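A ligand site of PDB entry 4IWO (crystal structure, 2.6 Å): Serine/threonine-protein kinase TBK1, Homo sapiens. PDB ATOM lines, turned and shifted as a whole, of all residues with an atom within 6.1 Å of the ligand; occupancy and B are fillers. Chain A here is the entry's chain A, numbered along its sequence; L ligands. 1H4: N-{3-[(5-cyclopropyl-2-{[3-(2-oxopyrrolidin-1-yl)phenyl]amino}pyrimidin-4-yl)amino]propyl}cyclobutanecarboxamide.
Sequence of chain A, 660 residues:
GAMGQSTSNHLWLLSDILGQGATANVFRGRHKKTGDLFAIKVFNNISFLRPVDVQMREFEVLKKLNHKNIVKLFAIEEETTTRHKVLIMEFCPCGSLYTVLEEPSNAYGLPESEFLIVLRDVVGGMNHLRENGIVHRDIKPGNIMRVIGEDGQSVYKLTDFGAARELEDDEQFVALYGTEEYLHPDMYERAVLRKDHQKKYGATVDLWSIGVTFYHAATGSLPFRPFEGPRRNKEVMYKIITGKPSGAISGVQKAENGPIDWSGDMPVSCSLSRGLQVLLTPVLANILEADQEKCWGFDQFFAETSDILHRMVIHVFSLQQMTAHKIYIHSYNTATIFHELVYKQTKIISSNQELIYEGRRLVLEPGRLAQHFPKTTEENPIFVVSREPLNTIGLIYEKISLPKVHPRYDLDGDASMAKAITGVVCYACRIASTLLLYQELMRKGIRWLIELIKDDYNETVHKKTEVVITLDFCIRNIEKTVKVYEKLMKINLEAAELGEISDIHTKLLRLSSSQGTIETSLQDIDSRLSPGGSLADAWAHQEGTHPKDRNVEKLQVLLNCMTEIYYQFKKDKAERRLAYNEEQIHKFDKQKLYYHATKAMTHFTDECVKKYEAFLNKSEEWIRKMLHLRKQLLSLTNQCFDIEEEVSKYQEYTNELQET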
ATOM      1  N   LEU A  18     -30.689  -0.523 -14.701  1.00  0.00           N
ATOM      2  CA  LEU A  18     -30.395  -1.952 -14.698  1.00  0.00           C
ATOM      3  C   LEU A  18     -31.649  -2.805 -14.835  1.00  0.00           C
ATOM      4  O   LEU A  18     -31.758  -3.617 -15.762  1.00  0.00           O
ATOM      5  CB  LEU A  18     -29.625  -2.336 -13.432  1.00  0.00           C
ATOM      6  CG  LEU A  18     -28.208  -1.763 -13.302  1.00  0.00           C
ATOM      7  CD1 LEU A  18     -27.568  -2.204 -11.996  1.00  0.00           C
ATOM      8  CD2 LEU A  18     -27.344  -2.163 -14.489  1.00  0.00           C
ATOM      9  N   GLY A  19     -32.556  -2.676 -13.883  1.00  0.00           N
ATOM     10  CA  GLY A  19     -33.785  -3.447 -13.881  1.00  0.00           C
ATOM     11  C   GLY A  19     -34.953  -2.623 -13.385  1.00  0.00           C
ATOM     12  O   GLY A  19     -34.786  -1.688 -12.606  1.00  0.00           O
ATOM     13  N   GLN A  20     -36.154  -2.982 -13.836  1.00  0.00           N
ATOM     14  CA  GLN A  20     -37.354  -2.307 -13.367  1.00  0.00           C
ATOM     15  C   GLN A  20     -38.251  -3.294 -12.633  1.00  0.00           C
ATOM     16  O   GLN A  20     -38.583  -4.357 -13.151  1.00  0.00           O
ATOM     17  CB  GLN A  20     -38.113  -1.692 -14.549  1.00  0.00           C
ATOM     18  CG  GLN A  20     -37.383  -0.536 -15.222  1.00  0.00           C
ATOM     19  CD  GLN A  20     -38.130   0.000 -16.428  1.00  0.00           C
ATOM     20  OE1 GLN A  20     -38.924  -0.712 -17.046  1.00  0.00           O
ATOM     21  NE2 GLN A  20     -37.875   1.259 -16.759  1.00  0.00           N
ATOM     22  N   GLY A  21     -38.631  -2.931 -11.408  1.00  0.00           N
ATOM     23  CA  GLY A  21     -39.541  -3.743 -10.630  1.00  0.00           C
ATOM     24  C   GLY A  21     -40.757  -2.958 -10.181  1.00  0.00           C
ATOM     25  O   GLY A  21     -40.873  -1.759 -10.447  1.00  0.00           O
ATOM     26  N   ALA A  22     -41.673  -3.637  -9.501  1.00  0.00           N
ATOM     27  CA  ALA A  22     -42.910  -3.011  -9.029  1.00  0.00           C
ATOM     28  C   ALA A  22     -42.612  -1.959  -7.961  1.00  0.00           C
ATOM     29  O   ALA A  22     -42.912  -0.777  -8.139  1.00  0.00           O
ATOM     30  CB  ALA A  22     -43.865  -4.066  -8.481  1.00  0.00           C
ATOM     31  N   ALA A  24     -39.540  -1.038  -6.643  1.00  0.00           N
ATOM     32  CA  ALA A  24     -38.354  -0.218  -6.827  1.00  0.00           C
ATOM     33  C   ALA A  24     -37.714  -0.346  -8.210  1.00  0.00           C
ATOM     34  O   ALA A  24     -38.081  -1.209  -9.002  1.00  0.00           O
ATOM     35  CB  ALA A  24     -37.326  -0.527  -5.752  1.00  0.00           C
ATOM     36  N   ASN A  25     -36.754   0.537  -8.473  1.00  0.00           N
ATOM     37  CA  ASN A  25     -35.925   0.467  -9.673  1.00  0.00           C
ATOM     38  C   ASN A  25     -34.466   0.332  -9.281  1.00  0.00           C
ATOM     39  O   ASN A  25     -34.069   0.692  -8.169  1.00  0.00           O
ATOM     40  CB  ASN A  25     -36.100   1.709 -10.536  1.00  0.00           C
ATOM     41  CG  ASN A  25     -37.554   2.003 -10.845  1.00  0.00           C
ATOM     42  OD1 ASN A  25     -38.401   1.114 -10.818  1.00  0.00           O
ATOM     43  ND2 ASN A  25     -37.844   3.260 -11.146  1.00  0.00           N
ATOM     44  N   VAL A  26     -33.654  -0.181 -10.210  1.00  0.00           N
ATOM     45  CA  VAL A  26     -32.222  -0.333  -9.966  1.00  0.00           C
ATOM     46  C   VAL A  26     -31.402   0.368 -11.041  1.00  0.00           C
ATOM     47  O   VAL A  26     -31.620   0.146 -12.233  1.00  0.00           O
ATOM     48  CB  VAL A  26     -31.811  -1.817  -9.885  1.00  0.00           C
ATOM     49  CG1 VAL A  26     -30.327  -1.938  -9.612  1.00  0.00           C
ATOM     50  CG2 VAL A  26     -32.615  -2.530  -8.811  1.00  0.00           C
ATOM     51  N   ARG A  28     -27.444   1.691 -12.536  1.00  0.00           N
ATOM     52  CA  ARG A  28     -25.991   1.593 -12.516  1.00  0.00           C
ATOM     53  C   ARG A  28     -25.437   2.903 -11.977  1.00  0.00           C
ATOM     54  O   ARG A  28     -25.601   3.954 -12.604  1.00  0.00           O
ATOM     55  CB  ARG A  28     -25.457   1.333 -13.925  1.00  0.00           C
ATOM     56  CG  ARG A  28     -23.949   1.203 -14.015  1.00  0.00           C
ATOM     57  CD  ARG A  28     -23.466   1.466 -15.436  1.00  0.00           C
ATOM     58  NE  ARG A  28     -22.064   1.098 -15.621  1.00  0.00           N
ATOM     59  CZ  ARG A  28     -21.663  -0.032 -16.175  1.00  0.00           C
ATOM     60  NH1 ARG A  28     -22.555  -0.926 -16.599  1.00  0.00           N
ATOM     61  NH2 ARG A  28     -20.366  -0.296 -16.311  1.00  0.00           N
ATOM     62  N   ALA A  39     -24.922  -1.198  -7.547  1.00  0.00           N
ATOM     63  CA  ALA A  39     -26.322  -1.234  -7.929  1.00  0.00           C
ATOM     64  C   ALA A  39     -27.145  -0.435  -6.920  1.00  0.00           C
ATOM     65  O   ALA A  39     -27.239  -0.789  -5.744  1.00  0.00           O
ATOM     66  CB  ALA A  39     -26.812  -2.679  -8.014  1.00  0.00           C
ATOM     67  N   ILE A  40     -27.752   0.648  -7.387  1.00  0.00           N
ATOM     68  CA  ILE A  40     -28.554   1.508  -6.523  1.00  0.00           C
ATOM     69  C   ILE A  40     -30.042   1.202  -6.671  1.00  0.00           C
ATOM     70  O   ILE A  40     -30.610   1.352  -7.752  1.00  0.00           O
ATOM     71  CB  ILE A  40     -28.293   3.010  -6.791  1.00  0.00           C
ATOM     72  CG1 ILE A  40     -26.961   3.452  -6.180  1.00  0.00           C
ATOM     73  CG2 ILE A  40     -29.408   3.843  -6.203  1.00  0.00           C
ATOM     74  CD1 ILE A  40     -25.742   3.105  -7.009  1.00  0.00           C
ATOM     75  N   LYS A  41     -30.664   0.768  -5.573  1.00  0.00           N
ATOM     76  CA  LYS A  41     -32.083   0.406  -5.584  1.00  0.00           C
ATOM     77  C   LYS A  41     -32.946   1.531  -5.016  1.00  0.00           C
ATOM     78  O   LYS A  41     -32.945   1.781  -3.807  1.00  0.00           O
ATOM     79  CB  LYS A  41     -32.302  -0.891  -4.805  1.00  0.00           C
ATOM     80  CG  LYS A  41     -33.724  -1.430  -4.866  1.00  0.00           C
ATOM     81  CD  LYS A  41     -33.832  -2.786  -4.183  1.00  0.00           C
ATOM     82  CE  LYS A  41     -35.248  -3.348  -4.263  1.00  0.00           C
ATOM     83  NZ  LYS A  41     -35.372  -4.672  -3.601  1.00  0.00           N
ATOM     84  N   VAL A  71     -26.643 -11.705  -3.464  1.00  0.00           N
ATOM     85  CA  VAL A  71     -26.155 -10.351  -3.737  1.00  0.00           C
ATOM     86  C   VAL A  71     -26.047  -9.535  -2.452  1.00  0.00           C
ATOM     87  O   VAL A  71     -27.000  -9.444  -1.682  1.00  0.00           O
ATOM     88  CB  VAL A  71     -27.058  -9.616  -4.733  1.00  0.00           C
ATOM     89  CG1 VAL A  71     -26.393  -8.326  -5.174  1.00  0.00           C
ATOM     90  CG2 VAL A  71     -27.354 -10.487  -5.936  1.00  0.00           C
ATOM     91  N   MET A  89     -26.512  -1.725  -3.422  1.00  0.00           N
ATOM     92  CA  MET A  89     -26.317  -3.140  -3.657  1.00  0.00           C
ATOM     93  C   MET A  89     -25.078  -3.443  -4.506  1.00  0.00           C
ATOM     94  O   MET A  89     -24.595  -2.578  -5.241  1.00  0.00           O
ATOM     95  CB  MET A  89     -27.548  -3.720  -4.353  1.00  0.00           C
ATOM     96  CG  MET A  89     -28.866  -3.419  -3.644  1.00  0.00           C
ATOM     97  SD  MET A  89     -29.242  -4.604  -2.347  1.00  0.00           S
ATOM     98  CE  MET A  89     -29.423  -6.103  -3.312  1.00  0.00           C
ATOM     99  N   GLU A  90     -24.589  -4.669  -4.388  1.00  0.00           N
ATOM    100  CA  GLU A  90     -23.480  -5.144  -5.192  1.00  0.00           C
ATOM    101  C   GLU A  90     -23.871  -5.193  -6.670  1.00  0.00           C
ATOM    102  O   GLU A  90     -24.913  -5.735  -7.017  1.00  0.00           O
ATOM    103  CB  GLU A  90     -23.061  -6.533  -4.725  1.00  0.00           C
ATOM    104  CG  GLU A  90     -22.252  -7.333  -5.731  1.00  0.00           C
ATOM    105  CD  GLU A  90     -22.070  -8.774  -5.316  1.00  0.00           C
ATOM    106  OE1 GLU A  90     -21.604  -9.578  -6.156  1.00  0.00           O
ATOM    107  OE2 GLU A  90     -22.379  -9.109  -4.154  1.00  0.00           O
ATOM    108  N   PHE A  91     -23.044  -4.608  -7.528  1.00  0.00           N
ATOM    109  CA  PHE A  91     -23.335  -4.552  -8.955  1.00  0.00           C
ATOM    110  C   PHE A  91     -22.868  -5.804  -9.691  1.00  0.00           C
ATOM    111  O   PHE A  91     -21.742  -6.276  -9.495  1.00  0.00           O
ATOM    112  CB  PHE A  91     -22.718  -3.301  -9.588  1.00  0.00           C
ATOM    113  CG  PHE A  91     -22.902  -3.215 -11.080  1.00  0.00           C
ATOM    114  CD1 PHE A  91     -24.151  -3.312 -11.646  1.00  0.00           C
ATOM    115  CD2 PHE A  91     -21.806  -3.020 -11.910  1.00  0.00           C
ATOM    116  CE1 PHE A  91     -24.317  -3.234 -13.017  1.00  0.00           C
ATOM    117  CE2 PHE A  91     -21.967  -2.935 -13.283  1.00  0.00           C
ATOM    118  CZ  PHE A  91     -23.225  -3.046 -13.836  1.00  0.00           C
ATOM    119  N   CYS A  92     -23.738  -6.342 -10.551  1.00  0.00           N
ATOM    120  CA  CYS A  92     -23.417  -7.532 -11.329  1.00  0.00           C
ATOM    121  C   CYS A  92     -23.457  -7.213 -12.834  1.00  0.00           C
ATOM    122  O   CYS A  92     -24.516  -7.274 -13.450  1.00  0.00           O
ATOM    123  CB  CYS A  92     -24.396  -8.656 -11.013  1.00  0.00           C
ATOM    124  SG  CYS A  92     -24.612  -8.978  -9.235  1.00  0.00           S
ATOM    125  N   PRO A  93     -22.288  -6.891 -13.406  1.00  0.00           N
ATOM    126  CA  PRO A  93     -22.162  -6.422 -14.786  1.00  0.00           C
ATOM    127  C   PRO A  93     -22.627  -7.411 -15.851  1.00  0.00           C
ATOM    128  O   PRO A  93     -23.011  -6.993 -16.946  1.00  0.00           O
ATOM    129  CB  PRO A  93     -20.653  -6.170 -14.931  1.00  0.00           C
ATOM    130  CG  PRO A  93     -20.022  -6.986 -13.855  1.00  0.00           C
ATOM    131  CD  PRO A  93     -20.989  -6.970 -12.726  1.00  0.00           C
ATOM    132  N   CYS A  94     -22.595  -8.705 -15.559  1.00  0.00           N
ATOM    133  CA  CYS A  94     -22.961  -9.723 -16.547  1.00  0.00           C
ATOM    134  C   CYS A  94     -24.464  -9.859 -16.775  1.00  0.00           C
ATOM    135  O   CYS A  94     -24.908 -10.477 -17.735  1.00  0.00           O
ATOM    136  CB  CYS A  94     -22.368 -11.091 -16.176  1.00  0.00           C
ATOM    137  SG  CYS A  94     -20.567 -11.146 -16.206  1.00  0.00           S
ATOM    138  N   GLY A  95     -25.250  -9.260 -15.882  1.00  0.00           N
ATOM    139  CA  GLY A  95     -26.702  -9.328 -15.994  1.00  0.00           C
ATOM    140  C   GLY A  95     -27.289 -10.450 -15.168  1.00  0.00           C
ATOM    141  O   GLY A  95     -26.832 -10.712 -14.054  1.00  0.00           O
ATOM    142  N   SER A  96     -28.311 -11.107 -15.699  1.00  0.00           N
ATOM    143  CA  SER A  96     -28.981 -12.177 -14.966  1.00  0.00           C
ATOM    144  C   SER A  96     -29.079 -13.458 -15.788  1.00  0.00           C
ATOM    145  O   SER A  96     -28.559 -13.526 -16.900  1.00  0.00           O
ATOM    146  CB  SER A  96     -30.373 -11.731 -14.506  1.00  0.00           C
ATOM    147  OG  SER A  96     -31.218 -11.493 -15.617  1.00  0.00           O
ATOM    148  N   THR A  99     -30.705 -12.839 -19.094  1.00  0.00           N
ATOM    149  CA  THR A  99     -29.765 -12.306 -20.069  1.00  0.00           C
ATOM    150  C   THR A  99     -28.975 -13.433 -20.715  1.00  0.00           C
ATOM    151  O   THR A  99     -28.643 -13.391 -21.898  1.00  0.00           O
ATOM    152  CB  THR A  99     -28.776 -11.333 -19.405  1.00  0.00           C
ATOM    153  OG1 THR A  99     -29.490 -10.368 -18.621  1.00  0.00           O
ATOM    154  CG2 THR A  99     -27.939 -10.613 -20.455  1.00  0.00           C
ATOM    155  N   GLY A 142     -34.932 -13.831 -14.056  1.00  0.00           N
ATOM    156  CA  GLY A 142     -34.783 -12.383 -13.970  1.00  0.00           C
ATOM    157  C   GLY A 142     -34.156 -11.895 -12.680  1.00  0.00           C
ATOM    158  O   GLY A 142     -33.441 -10.886 -12.677  1.00  0.00           O
ATOM    159  N   ASN A 143     -34.419 -12.588 -11.576  1.00  0.00           N
ATOM    160  CA  ASN A 143     -33.867 -12.196 -10.281  1.00  0.00           C
ATOM    161  C   ASN A 143     -32.682 -13.060  -9.844  1.00  0.00           C
ATOM    162  O   ASN A 143     -32.218 -12.974  -8.701  1.00  0.00           O
ATOM    163  CB  ASN A 143     -34.957 -12.167  -9.212  1.00  0.00           C
ATOM    164  CG  ASN A 143     -35.617 -13.522  -9.000  1.00  0.00           C
ATOM    165  OD1 ASN A 143     -34.945 -14.554  -8.837  1.00  0.00           O
ATOM    166  ND2 ASN A 143     -36.942 -13.540  -8.998  1.00  0.00           N
ATOM    167  N   MET A 145     -29.017 -13.335 -10.449  1.00  0.00           N
ATOM    168  CA  MET A 145     -27.907 -12.567 -11.012  1.00  0.00           C
ATOM    169  C   MET A 145     -26.717 -13.447 -11.362  1.00  0.00           C
ATOM    170  O   MET A 145     -26.558 -14.543 -10.821  1.00  0.00           O
ATOM    171  CB  MET A 145     -27.466 -11.469 -10.037  1.00  0.00           C
ATOM    172  CG  MET A 145     -28.625 -10.619  -9.514  1.00  0.00           C
ATOM    173  SD  MET A 145     -29.674  -9.999 -10.838  1.00  0.00           S
ATOM    174  CE  MET A 145     -28.495  -9.020 -11.767  1.00  0.00           C
ATOM    175  N   THR A 159     -31.452 -12.681  -5.488  1.00  0.00           N
ATOM    176  CA  THR A 159     -31.826 -11.319  -5.090  1.00  0.00           C
ATOM    177  C   THR A 159     -33.343 -11.127  -4.935  1.00  0.00           C
ATOM    178  O   THR A 159     -34.126 -11.982  -5.333  1.00  0.00           O
ATOM    179  CB  THR A 159     -31.287 -10.271  -6.094  1.00  0.00           C
ATOM    180  OG1 THR A 159     -31.469  -8.956  -5.562  1.00  0.00           O
ATOM    181  CG2 THR A 159     -32.024 -10.389  -7.418  1.00  0.00           C
ATOM    182  N   ASP A 160     -33.733  -9.986  -4.354  1.00  0.00           N
ATOM    183  CA  ASP A 160     -35.142  -9.585  -4.264  1.00  0.00           C
ATOM    184  C   ASP A 160     -36.137 -10.530  -3.557  1.00  0.00           C
ATOM    185  O   ASP A 160     -37.188 -10.849  -4.103  1.00  0.00           O
ATOM    186  CB  ASP A 160     -35.679  -9.230  -5.651  1.00  0.00           C
ATOM    187  CG  ASP A 160     -36.807  -8.220  -5.604  1.00  0.00           C
ATOM    188  OD1 ASP A 160     -36.822  -7.389  -4.676  1.00  0.00           O
ATOM    189  OD2 ASP A 160     -37.689  -8.267  -6.490  1.00  0.00           O
HETATM  190  C14 1H4 L   1     -29.622  -4.954  -7.119  1.00  0.00           C
HETATM  191  C11 1H4 L   1     -27.730  -6.072  -9.589  1.00  0.00           C
HETATM  192  C10 1H4 L   1     -27.614  -5.675 -11.716  1.00  0.00           C
HETATM  193  C12 1H4 L   1     -28.994  -5.981  -9.284  1.00  0.00           C
HETATM  194  C13 1H4 L   1     -29.584  -6.186  -7.849  1.00  0.00           C
HETATM  195  C01 1H4 L   1     -36.108  -5.766  -9.662  1.00  0.00           C
HETATM  196  C02 1H4 L   1     -35.883  -4.292  -9.255  1.00  0.00           C
HETATM  197  C03 1H4 L   1     -35.380  -4.813  -7.914  1.00  0.00           C
HETATM  198  C04 1H4 L   1     -35.441  -6.143  -8.471  1.00  0.00           C
HETATM  199  C05 1H4 L   1     -34.078  -6.662  -8.753  1.00  0.00           C
HETATM  200  O01 1H4 L   1     -33.347  -6.794  -7.572  1.00  0.00           O
HETATM  201  N01 1H4 L   1     -33.933  -6.840 -10.100  1.00  0.00           N
HETATM  202  C06 1H4 L   1     -32.861  -7.707 -10.594  1.00  0.00           C
HETATM  203  C07 1H4 L   1     -32.246  -7.082 -11.868  1.00  0.00           C
HETATM  204  C08 1H4 L   1     -32.042  -5.602 -11.601  1.00  0.00           C
HETATM  205  N02 1H4 L   1     -31.287  -5.462 -10.386  1.00  0.00           N
HETATM  206  C09 1H4 L   1     -29.850  -5.636 -10.457  1.00  0.00           C
HETATM  207  N03 1H4 L   1     -29.089  -5.465 -11.816  1.00  0.00           N
HETATM  208  N04 1H4 L   1     -27.202  -5.945 -10.613  1.00  0.00           N
HETATM  209  C15 1H4 L   1     -28.572  -6.003  -6.850  1.00  0.00           C
HETATM  210  N05 1H4 L   1     -26.721  -5.558 -12.847  1.00  0.00           N
HETATM  211  C16 1H4 L   1     -27.132  -5.709 -14.238  1.00  0.00           C
HETATM  212  C17 1H4 L   1     -26.069  -5.576 -15.454  1.00  0.00           C
HETATM  213  C18 1H4 L   1     -26.652  -5.756 -16.809  1.00  0.00           C
HETATM  214  C19 1H4 L   1     -27.896  -5.978 -16.809  1.00  0.00           C
HETATM  215  C20 1H4 L   1     -28.708  -6.089 -15.959  1.00  0.00           C
HETATM  216  C21 1H4 L   1     -28.552  -5.990 -14.679  1.00  0.00           C
HETATM  217  N   1H4 L   1     -25.870  -5.674 -18.008  1.00  0.00           N
HETATM  218  C22 1H4 L   1     -26.073  -6.475 -19.216  1.00  0.00           C
HETATM  219  C23 1H4 L   1     -25.095  -5.951 -20.259  1.00  0.00           C
HETATM  220  C24 1H4 L   1     -24.206  -4.976 -19.588  1.00  0.00           C
HETATM  221  C   1H4 L   1     -24.744  -4.765 -18.223  1.00  0.00           C
HETATM  222  O   1H4 L   1     -24.315  -3.955 -17.406  1.00  0.00           O
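O01 of the ligand is in hydrogen-bond range of OG1 of Thr 159, at 3.5 Å.
The backbone carbonyl oxygen (O) of Cys 92 sits at hydrogen-bond distance from a nitrogen (N05) of the ligand (2.9 Å).
N of Cys 92 is in hydrogen-bond range of N04 of the ligand.
O of Ala 39 sits at hydrogen-bond distance from N of Met 89 (2.6 Å).
O of Asn 143 sits close to N of Thr 159.
The backbone carbonyl oxygen (O) of Val 26 lies within hydrogen-bond range of the backbone NH (N) of Leu 18.
The side-chain carboxylate of Asp 160 is in salt-bridge range of the side-chain amino group of Lys 41 (3.3 Å).
O of Gly 19 is in hydrogen-bond range of N of Val 26 (3.0 Å).
O of Pro 93 lies close to N of the ligand, at 3.3 Å.
Leu 18 touches the ligand (CD1 to C10, 3.5 Å).
CA of Gly 19 touches C08 of the ligand, at 3.6 Å.
N of Gly 21 touches C02 of the ligand (3.7 Å).
Ala 24 touches the ligand (O to C02, 3.8 Å).
Val 26 touches the ligand (CG2 to N02, 3.6 Å).
Arg 28 touches the ligand (NH1 to O, 3.6 Å).
CB of Ala 39 touches C14 of the ligand, 3.7 Å away.
Lys 41 touches the ligand.
CG1 of Val 71 touches C15 of the ligand (3.6 Å).
Met 89 touches the ligand.
O of Glu 90 touches C15 of the ligand (3.7 Å).
Phe 91 touches the ligand (CE1 to N05, 3.3 Å).
CA of Gly 95 touches C19 of the ligand (3.6 Å).
Gly 142 touches the ligand (O to C06, 3.8 Å).
CE of Met 145 touches C10 of the ligand, 3.5 Å away.
Asp 160 touches the ligand (OD2 to C04, 3.7 Å).
Of the 27 residues printed, 19 come within 4 Å of the ligand.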
